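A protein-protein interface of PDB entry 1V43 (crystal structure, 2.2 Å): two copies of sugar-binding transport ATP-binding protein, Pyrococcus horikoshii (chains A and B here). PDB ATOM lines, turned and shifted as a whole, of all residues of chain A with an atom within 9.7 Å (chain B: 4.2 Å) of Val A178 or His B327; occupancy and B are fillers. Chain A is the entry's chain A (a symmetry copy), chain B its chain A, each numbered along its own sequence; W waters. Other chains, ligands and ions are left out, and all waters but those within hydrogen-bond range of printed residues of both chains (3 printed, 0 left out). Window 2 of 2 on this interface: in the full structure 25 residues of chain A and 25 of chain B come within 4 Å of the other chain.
Water W2 lies within hydrogen-bond range of O of Lys A175 (2.7 Å), NZ of Lys B336 (3.2 Å) and N of Ala A179 (3.3 Å). Water W1 lies within hydrogen-bond range of the side-chain hydroxyl (OG1) of Thr A207 (2.8 Å), the side-chain carboxylate (OE1) of Glu B318 (2.8 Å) and the guanidinium group (NH1) of Arg A181 (2.8 Å). Water W3 lies within hydrogen-bond range of the side-chain amino group (NZ) of Lys A186 (3.1 Å) and the side-chain carboxylate (OD1) of Asp B315 (3.3 Å).
Of the 24 printed residues of chain A, 5 touch a printed residue of chain B. Hydrophobic or aromatic side chains of chain A within 4 Å of the printed part of chain B: Val A178 and Ala A182. Among the printed residues, 8 pairs touch across the chains.
No position is printed for both chains. Of the 8 pairs that touch across the chains among the printed residues, none has its exchanged pair printed and touching as well.
OE2 of Glu B318 touches CG1 of Val A178, 3.4 Å away. Val A178 touches His B327. CG1 of Val A178 touches NZ of Lys B336, at 3.8 Å. Phe B316 touches Ala A182 (CD2 to CB, 3.7 Å). CG of Lys A185 touches CE1 of Phe B316, 3.9 Å away. Phe B316 touches Lys A186. Thr A207 touches Phe B316 (CG2 to CE2, 3.8 Å).
O of His B327 sits at hydrogen-bond distance from N of Asp B315, at 2.7 Å. The backbone carbonyl oxygen of Phe B316 lies within hydrogen-bond range of the backbone NH of His B327 (2.8 Å). The backbone NH (N) of Ile B325 lies within hydrogen-bond range of the backbone carbonyl oxygen (O) of Glu B318, at 2.8 Å. The side-chain carboxylate of Glu B318 lies within hydrogen-bond range of a ring nitrogen (NE2) of His B327, at 2.8 Å. The side-chain amino group (NZ) of Lys A185 lies within hydrogen-bond range of the backbone carbonyl oxygen (O) of Met A208, at 2.5 Å. The backbone carbonyl oxygen (O) of Val A203 sits at hydrogen-bond distance from the side-chain hydroxyl (OG1) of Thr A207.
Of chain B, only Glu B318, His B327 and Lys B336 come within 4 Å of Val A178. His B327 touches one residue of chain A. No residue of chain A comes within 4 Å of Val B314. No residue of chain A comes within 4 Å of Val B328. Of the printed residues of chain A, Phe B316 touches Ala A182, Lys A185, Lys A186 and Thr A207. Printed residues of chain B within 4 Å of Lys A186: Asp B315 and Phe B316. The nearest printed residue of chain B that does not touch Val A178 is Phe B316 (5.6 Å). The nearest residue of chain A that does not touch His B327 is Ala A182 (4.6 Å).
OD2 of Asp B315 is in salt-bridge range of NZ of Lys A186 (2.4 Å).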
ATOM      1  N   GLN A 146     -12.245  -8.180 -29.487  1.00  0.00           N
ATOM      2  CA  GLN A 146     -11.583  -9.076 -28.552  1.00  0.00           C
ATOM      3  C   GLN A 146     -12.568 -10.128 -28.063  1.00  0.00           C
ATOM      4  O   GLN A 146     -13.693  -9.809 -27.669  1.00  0.00           O
ATOM      5  CB  GLN A 146     -11.033  -8.287 -27.357  1.00  0.00           C
ATOM      6  CG  GLN A 146     -10.208  -7.074 -27.755  1.00  0.00           C
ATOM      7  CD  GLN A 146      -9.699  -6.268 -26.569  1.00  0.00           C
ATOM      8  OE1 GLN A 146     -10.464  -5.867 -25.687  1.00  0.00           O
ATOM      9  NE2 GLN A 146      -8.396  -6.017 -26.551  1.00  0.00           N
ATOM     10  N   GLN A 148     -12.101 -11.556 -25.590  1.00  0.00           N
ATOM     11  CA  GLN A 148     -12.067 -11.312 -24.156  1.00  0.00           C
ATOM     12  C   GLN A 148     -13.297 -10.494 -23.776  1.00  0.00           C
ATOM     13  O   GLN A 148     -14.052 -10.855 -22.871  1.00  0.00           O
ATOM     14  CB  GLN A 148     -10.800 -10.546 -23.777  1.00  0.00           C
ATOM     15  CG  GLN A 148     -10.553 -10.493 -22.275  1.00  0.00           C
ATOM     16  CD  GLN A 148     -10.413 -11.870 -21.648  1.00  0.00           C
ATOM     17  OE1 GLN A 148      -9.556 -12.662 -22.050  1.00  0.00           O
ATOM     18  NE2 GLN A 148     -11.257 -12.163 -20.658  1.00  0.00           N
ATOM     19  N   LEU A 169      -7.482 -13.133 -16.751  1.00  0.00           N
ATOM     20  CA  LEU A 169      -6.512 -12.632 -17.711  1.00  0.00           C
ATOM     21  C   LEU A 169      -5.152 -13.328 -17.756  1.00  0.00           C
ATOM     22  O   LEU A 169      -4.235 -12.833 -18.407  1.00  0.00           O
ATOM     23  CB  LEU A 169      -6.298 -11.145 -17.426  1.00  0.00           C
ATOM     24  CG  LEU A 169      -7.258 -10.051 -17.922  1.00  0.00           C
ATOM     25  CD1 LEU A 169      -8.645 -10.562 -18.251  1.00  0.00           C
ATOM     26  CD2 LEU A 169      -7.299  -8.980 -16.867  1.00  0.00           C
ATOM     27  N   LEU A 172      -2.816 -13.783 -21.481  1.00  0.00           N
ATOM     28  CA  LEU A 172      -2.887 -12.654 -22.415  1.00  0.00           C
ATOM     29  C   LEU A 172      -1.537 -11.917 -22.461  1.00  0.00           C
ATOM     30  O   LEU A 172      -0.849 -11.820 -21.446  1.00  0.00           O
ATOM     31  CB  LEU A 172      -3.998 -11.675 -21.993  1.00  0.00           C
ATOM     32  CG  LEU A 172      -5.467 -12.047 -22.248  1.00  0.00           C
ATOM     33  CD1 LEU A 172      -5.830 -13.323 -21.517  1.00  0.00           C
ATOM     34  CD2 LEU A 172      -6.365 -10.918 -21.793  1.00  0.00           C
ATOM     35  N   ASP A 173      -1.157 -11.406 -23.631  1.00  0.00           N
ATOM     36  CA  ASP A 173       0.110 -10.691 -23.753  1.00  0.00           C
ATOM     37  C   ASP A 173       0.086  -9.470 -22.843  1.00  0.00           C
ATOM     38  O   ASP A 173      -0.942  -8.815 -22.689  1.00  0.00           O
ATOM     39  CB  ASP A 173       0.391 -10.280 -25.217  1.00  0.00           C
ATOM     40  CG  ASP A 173      -0.708  -9.400 -25.826  1.00  0.00           C
ATOM     41  OD1 ASP A 173      -1.738  -9.944 -26.284  1.00  0.00           O
ATOM     42  OD2 ASP A 173      -0.539  -8.160 -25.853  1.00  0.00           O
ATOM     43  N   ALA A 174       1.224  -9.183 -22.227  1.00  0.00           N
ATOM     44  CA  ALA A 174       1.347  -8.066 -21.300  1.00  0.00           C
ATOM     45  C   ALA A 174       0.584  -6.814 -21.709  1.00  0.00           C
ATOM     46  O   ALA A 174      -0.138  -6.232 -20.899  1.00  0.00           O
ATOM     47  CB  ALA A 174       2.816  -7.737 -21.087  1.00  0.00           C
ATOM     48  N   LYS A 175       0.736  -6.399 -22.963  1.00  0.00           N
ATOM     49  CA  LYS A 175       0.066  -5.196 -23.459  1.00  0.00           C
ATOM     50  C   LYS A 175      -1.466  -5.321 -23.467  1.00  0.00           C
ATOM     51  O   LYS A 175      -2.187  -4.385 -23.082  1.00  0.00           O
ATOM     52  CB  LYS A 175       0.590  -4.863 -24.858  1.00  0.00           C
ATOM     53  CG  LYS A 175       0.021  -3.606 -25.511  1.00  0.00           C
ATOM     54  CD  LYS A 175       0.602  -3.465 -26.929  1.00  0.00           C
ATOM     55  CE  LYS A 175      -0.063  -2.364 -27.729  1.00  0.00           C
ATOM     56  NZ  LYS A 175       0.587  -2.168 -29.059  1.00  0.00           N
ATOM     57  N   LEU A 176      -1.968  -6.470 -23.900  1.00  0.00           N
ATOM     58  CA  LEU A 176      -3.407  -6.679 -23.927  1.00  0.00           C
ATOM     59  C   LEU A 176      -3.936  -6.849 -22.505  1.00  0.00           C
ATOM     60  O   LEU A 176      -5.055  -6.462 -22.203  1.00  0.00           O
ATOM     61  CB  LEU A 176      -3.755  -7.909 -24.760  1.00  0.00           C
ATOM     62  CG  LEU A 176      -5.229  -8.330 -24.763  1.00  0.00           C
ATOM     63  CD1 LEU A 176      -6.109  -7.223 -25.352  1.00  0.00           C
ATOM     64  CD2 LEU A 176      -5.376  -9.620 -25.565  1.00  0.00           C
ATOM     65  N   ARG A 177      -3.125  -7.421 -21.626  1.00  0.00           N
ATOM     66  CA  ARG A 177      -3.567  -7.619 -20.258  1.00  0.00           C
ATOM     67  C   ARG A 177      -3.875  -6.268 -19.601  1.00  0.00           C
ATOM     68  O   ARG A 177      -4.937  -6.104 -18.999  1.00  0.00           O
ATOM     69  CB  ARG A 177      -2.516  -8.400 -19.462  1.00  0.00           C
ATOM     70  CG  ARG A 177      -3.025  -8.912 -18.128  1.00  0.00           C
ATOM     71  CD  ARG A 177      -2.196 -10.069 -17.581  1.00  0.00           C
ATOM     72  NE  ARG A 177      -2.687 -10.478 -16.265  1.00  0.00           N
ATOM     73  CZ  ARG A 177      -2.254 -11.534 -15.589  1.00  0.00           C
ATOM     74  NH1 ARG A 177      -1.313 -12.309 -16.099  1.00  0.00           N
ATOM     75  NH2 ARG A 177      -2.763 -11.812 -14.396  1.00  0.00           N
ATOM     76  N   VAL A 178      -2.975  -5.294 -19.746  1.00  0.00           N
ATOM     77  CA  VAL A 178      -3.193  -3.983 -19.155  1.00  0.00           C
ATOM     78  C   VAL A 178      -4.458  -3.345 -19.707  1.00  0.00           C
ATOM     79  O   VAL A 178      -5.246  -2.762 -18.956  1.00  0.00           O
ATOM     80  CB  VAL A 178      -1.975  -3.037 -19.377  1.00  0.00           C
ATOM     81  CG1 VAL A 178      -2.368  -1.596 -19.081  1.00  0.00           C
ATOM     82  CG2 VAL A 178      -0.837  -3.425 -18.426  1.00  0.00           C
ATOM     83  N   ALA A 179      -4.657  -3.461 -21.019  1.00  0.00           N
ATOM     84  CA  ALA A 179      -5.851  -2.915 -21.656  1.00  0.00           C
ATOM     85  C   ALA A 179      -7.118  -3.564 -21.068  1.00  0.00           C
ATOM     86  O   ALA A 179      -8.120  -2.890 -20.855  1.00  0.00           O
ATOM     87  CB  ALA A 179      -5.786  -3.140 -23.179  1.00  0.00           C
ATOM     88  N   MET A 180      -7.068  -4.870 -20.814  1.00  0.00           N
ATOM     89  CA  MET A 180      -8.210  -5.578 -20.229  1.00  0.00           C
ATOM     90  C   MET A 180      -8.465  -5.151 -18.762  1.00  0.00           C
ATOM     91  O   MET A 180      -9.619  -4.965 -18.364  1.00  0.00           O
ATOM     92  CB  MET A 180      -8.002  -7.097 -20.299  1.00  0.00           C
ATOM     93  CG  MET A 180      -8.289  -7.736 -21.661  1.00  0.00           C
ATOM     94  SD  MET A 180      -9.816  -7.146 -22.471  1.00  0.00           S
ATOM     95  CE  MET A 180     -11.041  -7.620 -21.279  1.00  0.00           C
ATOM     96  N   ARG A 181      -7.406  -5.000 -17.965  1.00  0.00           N
ATOM     97  CA  ARG A 181      -7.561  -4.564 -16.572  1.00  0.00           C
ATOM     98  C   ARG A 181      -8.354  -3.271 -16.554  1.00  0.00           C
ATOM     99  O   ARG A 181      -9.364  -3.162 -15.861  1.00  0.00           O
ATOM    100  CB  ARG A 181      -6.204  -4.318 -15.917  1.00  0.00           C
ATOM    101  CG  ARG A 181      -5.426  -5.582 -15.619  1.00  0.00           C
ATOM    102  CD  ARG A 181      -4.017  -5.278 -15.199  1.00  0.00           C
ATOM    103  NE  ARG A 181      -3.222  -6.493 -15.134  1.00  0.00           N
ATOM    104  CZ  ARG A 181      -1.894  -6.503 -15.176  1.00  0.00           C
ATOM    105  NH1 ARG A 181      -1.227  -5.356 -15.283  1.00  0.00           N
ATOM    106  NH2 ARG A 181      -1.235  -7.652 -15.132  1.00  0.00           N
ATOM    107  N   ALA A 182      -7.898  -2.296 -17.335  1.00  0.00           N
ATOM    108  CA  ALA A 182      -8.567  -1.008 -17.419  1.00  0.00           C
ATOM    109  C   ALA A 182     -10.001  -1.168 -17.905  1.00  0.00           C
ATOM    110  O   ALA A 182     -10.919  -0.563 -17.355  1.00  0.00           O
ATOM    111  CB  ALA A 182      -7.801  -0.072 -18.352  1.00  0.00           C
ATOM    112  N   GLU A 183     -10.190  -1.956 -18.956  1.00  0.00           N
ATOM    113  CA  GLU A 183     -11.525  -2.189 -19.504  1.00  0.00           C
ATOM    114  C   GLU A 183     -12.463  -2.759 -18.422  1.00  0.00           C
ATOM    115  O   GLU A 183     -13.520  -2.216 -18.160  1.00  0.00           O
ATOM    116  CB  GLU A 183     -11.415  -3.166 -20.677  1.00  0.00           C
ATOM    117  CG  GLU A 183     -12.727  -3.520 -21.347  1.00  0.00           C
ATOM    118  CD  GLU A 183     -13.427  -2.318 -21.929  1.00  0.00           C
ATOM    119  OE1 GLU A 183     -12.744  -1.297 -22.177  1.00  0.00           O
ATOM    120  OE2 GLU A 183     -14.659  -2.395 -22.152  1.00  0.00           O
ATOM    121  N   ILE A 184     -12.053  -3.842 -17.773  1.00  0.00           N
ATOM    122  CA  ILE A 184     -12.872  -4.449 -16.733  1.00  0.00           C
ATOM    123  C   ILE A 184     -13.167  -3.493 -15.556  1.00  0.00           C
ATOM    124  O   ILE A 184     -14.327  -3.356 -15.147  1.00  0.00           O
ATOM    125  CB  ILE A 184     -12.225  -5.771 -16.256  1.00  0.00           C
ATOM    126  CG1 ILE A 184     -12.434  -6.837 -17.340  1.00  0.00           C
ATOM    127  CG2 ILE A 184     -12.822  -6.229 -14.902  1.00  0.00           C
ATOM    128  CD1 ILE A 184     -11.556  -8.073 -17.199  1.00  0.00           C
ATOM    129  N   LYS A 185     -12.141  -2.805 -15.058  1.00  0.00           N
ATOM    130  CA  LYS A 185     -12.301  -1.876 -13.945  1.00  0.00           C
ATOM    131  C   LYS A 185     -13.277  -0.737 -14.270  1.00  0.00           C
ATOM    132  O   LYS A 185     -14.189  -0.445 -13.489  1.00  0.00           O
ATOM    133  CB  LYS A 185     -10.932  -1.313 -13.521  1.00  0.00           C
ATOM    134  CG  LYS A 185     -10.981  -0.405 -12.273  1.00  0.00           C
ATOM    135  CD  LYS A 185     -11.949  -0.949 -11.215  1.00  0.00           C
ATOM    136  CE  LYS A 185     -12.072  -0.045 -10.003  1.00  0.00           C
ATOM    137  NZ  LYS A 185     -11.005  -0.287  -9.006  1.00  0.00           N
ATOM    138  N   LYS A 186     -13.109  -0.099 -15.426  1.00  0.00           N
ATOM    139  CA  LYS A 186     -14.020   0.982 -15.806  1.00  0.00           C
ATOM    140  C   LYS A 186     -15.455   0.493 -15.947  1.00  0.00           C
ATOM    141  O   LYS A 186     -16.388   1.187 -15.562  1.00  0.00           O
ATOM    142  CB  LYS A 186     -13.599   1.613 -17.121  1.00  0.00           C
ATOM    143  CG  LYS A 186     -12.314   2.410 -17.083  1.00  0.00           C
ATOM    144  CD  LYS A 186     -12.088   2.880 -18.507  1.00  0.00           C
ATOM    145  CE  LYS A 186     -10.817   3.643 -18.702  1.00  0.00           C
ATOM    146  NZ  LYS A 186     -10.676   3.903 -20.170  1.00  0.00           N
ATOM    147  N   TYR A 197     -12.718 -10.444  -7.153  1.00  0.00           N
ATOM    148  CA  TYR A 197     -11.727 -10.808  -8.159  1.00  0.00           C
ATOM    149  C   TYR A 197     -10.509 -11.510  -7.577  1.00  0.00           C
ATOM    150  O   TYR A 197      -9.822 -10.965  -6.715  1.00  0.00           O
ATOM    151  CB  TYR A 197     -11.297  -9.514  -8.850  1.00  0.00           C
ATOM    152  CG  TYR A 197     -10.552  -9.635 -10.155  1.00  0.00           C
ATOM    153  CD1 TYR A 197     -11.198  -9.389 -11.375  1.00  0.00           C
ATOM    154  CD2 TYR A 197      -9.184  -9.894 -10.176  1.00  0.00           C
ATOM    155  CE1 TYR A 197     -10.491  -9.389 -12.581  1.00  0.00           C
ATOM    156  CE2 TYR A 197      -8.466  -9.893 -11.377  1.00  0.00           C
ATOM    157  CZ  TYR A 197      -9.131  -9.637 -12.568  1.00  0.00           C
ATOM    158  OH  TYR A 197      -8.418  -9.609 -13.729  1.00  0.00           O
ATOM    159  N   ASP A 201      -1.443 -12.050  -9.009  1.00  0.00           N
ATOM    160  CA  ASP A 201      -0.637 -10.975  -9.607  1.00  0.00           C
ATOM    161  C   ASP A 201      -0.812  -9.630  -8.871  1.00  0.00           C
ATOM    162  O   ASP A 201      -1.812  -8.922  -9.080  1.00  0.00           O
ATOM    163  CB  ASP A 201      -1.052 -10.822 -11.079  1.00  0.00           C
ATOM    164  CG  ASP A 201      -0.114  -9.929 -11.873  1.00  0.00           C
ATOM    165  OD1 ASP A 201       0.184  -8.800 -11.428  1.00  0.00           O
ATOM    166  OD2 ASP A 201       0.311 -10.360 -12.961  1.00  0.00           O
ATOM    167  N   VAL A 203       0.568  -6.628  -9.243  1.00  0.00           N
ATOM    168  CA  VAL A 203       0.357  -5.428 -10.066  1.00  0.00           C
ATOM    169  C   VAL A 203      -1.101  -5.331 -10.532  1.00  0.00           C
ATOM    170  O   VAL A 203      -1.685  -4.244 -10.548  1.00  0.00           O
ATOM    171  CB  VAL A 203       1.269  -5.391 -11.316  1.00  0.00           C
ATOM    172  CG1 VAL A 203       0.775  -4.312 -12.291  1.00  0.00           C
ATOM    173  CG2 VAL A 203       2.728  -5.086 -10.897  1.00  0.00           C
ATOM    174  N   GLU A 204      -1.687  -6.465 -10.908  1.00  0.00           N
ATOM    175  CA  GLU A 204      -3.078  -6.487 -11.370  1.00  0.00           C
ATOM    176  C   GLU A 204      -3.992  -6.129 -10.197  1.00  0.00           C
ATOM    177  O   GLU A 204      -4.935  -5.360 -10.338  1.00  0.00           O
ATOM    178  CB  GLU A 204      -3.427  -7.877 -11.915  1.00  0.00           C
ATOM    179  CG  GLU A 204      -4.826  -8.016 -12.530  1.00  0.00           C
ATOM    180  CD  GLU A 204      -4.898  -9.186 -13.516  1.00  0.00           C
ATOM    181  OE1 GLU A 204      -4.145  -9.150 -14.510  1.00  0.00           O
ATOM    182  OE2 GLU A 204      -5.692 -10.129 -13.306  1.00  0.00           O
ATOM    183  N   THR A 207      -3.959  -2.503  -9.514  1.00  0.00           N
ATOM    184  CA  THR A 207      -4.604  -1.805 -10.623  1.00  0.00           C
ATOM    185  C   THR A 207      -6.116  -1.866 -10.571  1.00  0.00           C
ATOM    186  O   THR A 207      -6.803  -0.901 -10.916  1.00  0.00           O
ATOM    187  CB  THR A 207      -4.232  -2.417 -11.981  1.00  0.00           C
ATOM    188  OG1 THR A 207      -2.807  -2.466 -12.123  1.00  0.00           O
ATOM    189  CG2 THR A 207      -4.851  -1.607 -13.099  1.00  0.00           C
ATOM    190  N   MET A 208      -6.647  -2.998 -10.137  1.00  0.00           N
ATOM    191  CA  MET A 208      -8.087  -3.146 -10.160  1.00  0.00           C
ATOM    192  C   MET A 208      -8.931  -3.022  -8.892  1.00  0.00           C
ATOM    193  O   MET A 208     -10.073  -2.567  -8.951  1.00  0.00           O
ATOM    194  CB  MET A 208      -8.396  -4.464 -10.867  1.00  0.00           C
ATOM    195  CG  MET A 208      -7.915  -4.458 -12.334  1.00  0.00           C
ATOM    196  SD  MET A 208      -8.069  -6.074 -13.047  1.00  0.00           S
ATOM    197  CE  MET A 208      -9.644  -5.835 -13.925  1.00  0.00           C
ATOM    198  N   VAL B 314      -6.962  12.615 -17.876  1.00  0.00           N
ATOM    199  CA  VAL B 314      -6.556  11.288 -17.454  1.00  0.00           C
ATOM    200  C   VAL B 314      -7.721  10.336 -17.661  1.00  0.00           C
ATOM    201  O   VAL B 314      -8.789  10.529 -17.094  1.00  0.00           O
ATOM    202  CB  VAL B 314      -6.201  11.261 -15.963  1.00  0.00           C
ATOM    203  CG1 VAL B 314      -5.827   9.851 -15.556  1.00  0.00           C
ATOM    204  CG2 VAL B 314      -5.067  12.229 -15.680  1.00  0.00           C
ATOM    205  N   ASP B 315      -7.508   9.310 -18.468  1.00  0.00           N
ATOM    206  CA  ASP B 315      -8.535   8.319 -18.741  1.00  0.00           C
ATOM    207  C   ASP B 315      -8.498   7.151 -17.746  1.00  0.00           C
ATOM    208  O   ASP B 315      -9.526   6.543 -17.450  1.00  0.00           O
ATOM    209  CB  ASP B 315      -8.349   7.781 -20.152  1.00  0.00           C
ATOM    210  CG  ASP B 315      -9.426   6.803 -20.545  1.00  0.00           C
ATOM    211  OD1 ASP B 315     -10.602   7.212 -20.613  1.00  0.00           O
ATOM    212  OD2 ASP B 315      -9.093   5.630 -20.784  1.00  0.00           O
ATOM    213  N   PHE B 316      -7.312   6.826 -17.246  1.00  0.00           N
ATOM    214  CA  PHE B 316      -7.171   5.725 -16.295  1.00  0.00           C
ATOM    215  C   PHE B 316      -5.822   5.783 -15.597  1.00  0.00           C
ATOM    216  O   PHE B 316      -4.839   6.307 -16.140  1.00  0.00           O
ATOM    217  CB  PHE B 316      -7.313   4.381 -17.003  1.00  0.00           C
ATOM    218  CG  PHE B 316      -7.377   3.202 -16.066  1.00  0.00           C
ATOM    219  CD1 PHE B 316      -8.513   2.973 -15.284  1.00  0.00           C
ATOM    220  CD2 PHE B 316      -6.316   2.305 -15.982  1.00  0.00           C
ATOM    221  CE1 PHE B 316      -8.595   1.866 -14.431  1.00  0.00           C
ATOM    222  CE2 PHE B 316      -6.385   1.187 -15.130  1.00  0.00           C
ATOM    223  CZ  PHE B 316      -7.529   0.972 -14.355  1.00  0.00           C
ATOM    224  N   GLU B 318      -2.945   3.483 -13.238  1.00  0.00           N
ATOM    225  CA  GLU B 318      -2.413   2.254 -12.688  1.00  0.00           C
ATOM    226  C   GLU B 318      -1.551   2.772 -11.521  1.00  0.00           C
ATOM    227  O   GLU B 318      -0.400   3.147 -11.726  1.00  0.00           O
ATOM    228  CB  GLU B 318      -1.501   1.532 -13.691  1.00  0.00           C
ATOM    229  CG  GLU B 318      -2.133   1.089 -14.994  1.00  0.00           C
ATOM    230  CD  GLU B 318      -1.114   0.411 -15.912  1.00  0.00           C
ATOM    231  OE1 GLU B 318      -0.453  -0.541 -15.458  1.00  0.00           O
ATOM    232  OE2 GLU B 318      -0.961   0.820 -17.081  1.00  0.00           O
ATOM    233  N   ILE B 325       1.221   4.708 -13.413  1.00  0.00           N
ATOM    234  CA  ILE B 325       1.071   4.872 -14.856  1.00  0.00           C
ATOM    235  C   ILE B 325      -0.247   5.522 -15.257  1.00  0.00           C
ATOM    236  O   ILE B 325      -1.331   4.980 -15.017  1.00  0.00           O
ATOM    237  CB  ILE B 325       1.190   3.534 -15.589  1.00  0.00           C
ATOM    238  CG1 ILE B 325       2.484   2.850 -15.167  1.00  0.00           C
ATOM    239  CG2 ILE B 325       1.197   3.771 -17.120  1.00  0.00           C
ATOM    240  CD1 ILE B 325       2.685   1.499 -15.794  1.00  0.00           C
ATOM    241  N   LEU B 326      -0.145   6.682 -15.891  1.00  0.00           N
ATOM    242  CA  LEU B 326      -1.331   7.412 -16.322  1.00  0.00           C
ATOM    243  C   LEU B 326      -1.631   7.203 -17.799  1.00  0.00           C
ATOM    244  O   LEU B 326      -0.730   7.282 -18.639  1.00  0.00           O
ATOM    245  CB  LEU B 326      -1.142   8.910 -16.097  1.00  0.00           C
ATOM    246  CG  LEU B 326      -0.606   9.380 -14.751  1.00  0.00           C
ATOM    247  CD1 LEU B 326      -0.458  10.904 -14.800  1.00  0.00           C
ATOM    248  CD2 LEU B 326      -1.537   8.949 -13.627  1.00  0.00           C
ATOM    249  N   HIS B 327      -2.897   6.931 -18.107  1.00  0.00           N
ATOM    250  CA  HIS B 327      -3.331   6.778 -19.491  1.00  0.00           C
ATOM    251  C   HIS B 327      -4.015   8.112 -19.756  1.00  0.00           C
ATOM    252  O   HIS B 327      -5.121   8.357 -19.274  1.00  0.00           O
ATOM    253  CB  HIS B 327      -4.321   5.622 -19.643  1.00  0.00           C
ATOM    254  CG  HIS B 327      -3.789   4.297 -19.179  1.00  0.00           C
ATOM    255  ND1 HIS B 327      -4.402   3.102 -19.486  1.00  0.00           N
ATOM    256  CD2 HIS B 327      -2.729   3.982 -18.394  1.00  0.00           C
ATOM    257  CE1 HIS B 327      -3.745   2.108 -18.914  1.00  0.00           C
ATOM    258  NE2 HIS B 327      -2.726   2.615 -18.244  1.00  0.00           N
ATOM    259  N   VAL B 328      -3.325   8.987 -20.488  1.00  0.00           N
ATOM    260  CA  VAL B 328      -3.830  10.315 -20.786  1.00  0.00           C
ATOM    261  C   VAL B 328      -4.260  10.445 -22.231  1.00  0.00           C
ATOM    262  O   VAL B 328      -3.554  10.002 -23.139  1.00  0.00           O
ATOM    263  CB  VAL B 328      -2.759  11.396 -20.535  1.00  0.00           C
ATOM    264  CG1 VAL B 328      -3.403  12.775 -20.585  1.00  0.00           C
ATOM    265  CG2 VAL B 328      -2.080  11.168 -19.209  1.00  0.00           C
ATOM    266  N   LYS B 329      -5.419  11.062 -22.436  1.00  0.00           N
ATOM    267  CA  LYS B 329      -5.938  11.269 -23.777  1.00  0.00           C
ATOM    268  C   LYS B 329      -5.304  12.496 -24.410  1.00  0.00           C
ATOM    269  O   LYS B 329      -5.498  13.608 -23.940  1.00  0.00           O
ATOM    270  CB  LYS B 329      -7.457  11.458 -23.752  1.00  0.00           C
ATOM    271  CG  LYS B 329      -8.266  10.199 -23.480  1.00  0.00           C
ATOM    272  CD  LYS B 329      -9.752  10.485 -23.672  1.00  0.00           C
ATOM    273  CE  LYS B 329     -10.629   9.277 -23.370  1.00  0.00           C
ATOM    274  NZ  LYS B 329     -12.078   9.599 -23.554  1.00  0.00           N
ATOM    275  N   LEU B 334      -4.529   8.224 -27.201  1.00  0.00           N
ATOM    276  CA  LEU B 334      -4.352   7.752 -25.828  1.00  0.00           C
ATOM    277  C   LEU B 334      -2.902   7.303 -25.622  1.00  0.00           C
ATOM    278  O   LEU B 334      -2.425   6.392 -26.300  1.00  0.00           O
ATOM    279  CB  LEU B 334      -5.302   6.585 -25.564  1.00  0.00           C
ATOM    280  CG  LEU B 334      -5.507   6.132 -24.120  1.00  0.00           C
ATOM    281  CD1 LEU B 334      -5.997   7.294 -23.269  1.00  0.00           C
ATOM    282  CD2 LEU B 334      -6.523   4.998 -24.101  1.00  0.00           C
ATOM    283  N   VAL B 335      -2.201   7.946 -24.695  1.00  0.00           N
ATOM    284  CA  VAL B 335      -0.810   7.592 -24.427  1.00  0.00           C
ATOM    285  C   VAL B 335      -0.614   7.298 -22.949  1.00  0.00           C
ATOM    286  O   VAL B 335      -1.442   7.677 -22.119  1.00  0.00           O
ATOM    287  CB  VAL B 335       0.167   8.729 -24.825  1.00  0.00           C
ATOM    288  CG1 VAL B 335      -0.025   9.105 -26.288  1.00  0.00           C
ATOM    289  CG2 VAL B 335      -0.042   9.935 -23.925  1.00  0.00           C
ATOM    290  N   LYS B 336       0.483   6.623 -22.621  1.00  0.00           N
ATOM    291  CA  LYS B 336       0.782   6.299 -21.227  1.00  0.00           C
ATOM    292  C   LYS B 336       1.932   7.139 -20.735  1.00  0.00           C
ATOM    293  O   LYS B 336       2.902   7.342 -21.452  1.00  0.00           O
ATOM    294  CB  LYS B 336       1.169   4.829 -21.071  1.00  0.00           C
ATOM    295  CG  LYS B 336       0.069   3.846 -21.392  1.00  0.00           C
ATOM    296  CD  LYS B 336       0.601   2.438 -21.272  1.00  0.00           C
ATOM    297  CE  LYS B 336      -0.435   1.404 -21.633  1.00  0.00           C
ATOM    298  NZ  LYS B 336       0.121   0.039 -21.438  1.00  0.00           N
HETATM  299  O   HOH W   1      -2.030  -2.728 -14.768  1.00  0.00           O
HETATM  300  O   HOH W   2      -2.331  -1.718 -22.586  1.00  0.00           O
HETATM  301  O   HOH W   3     -12.943   5.199 -21.823  1.00  0.00           O
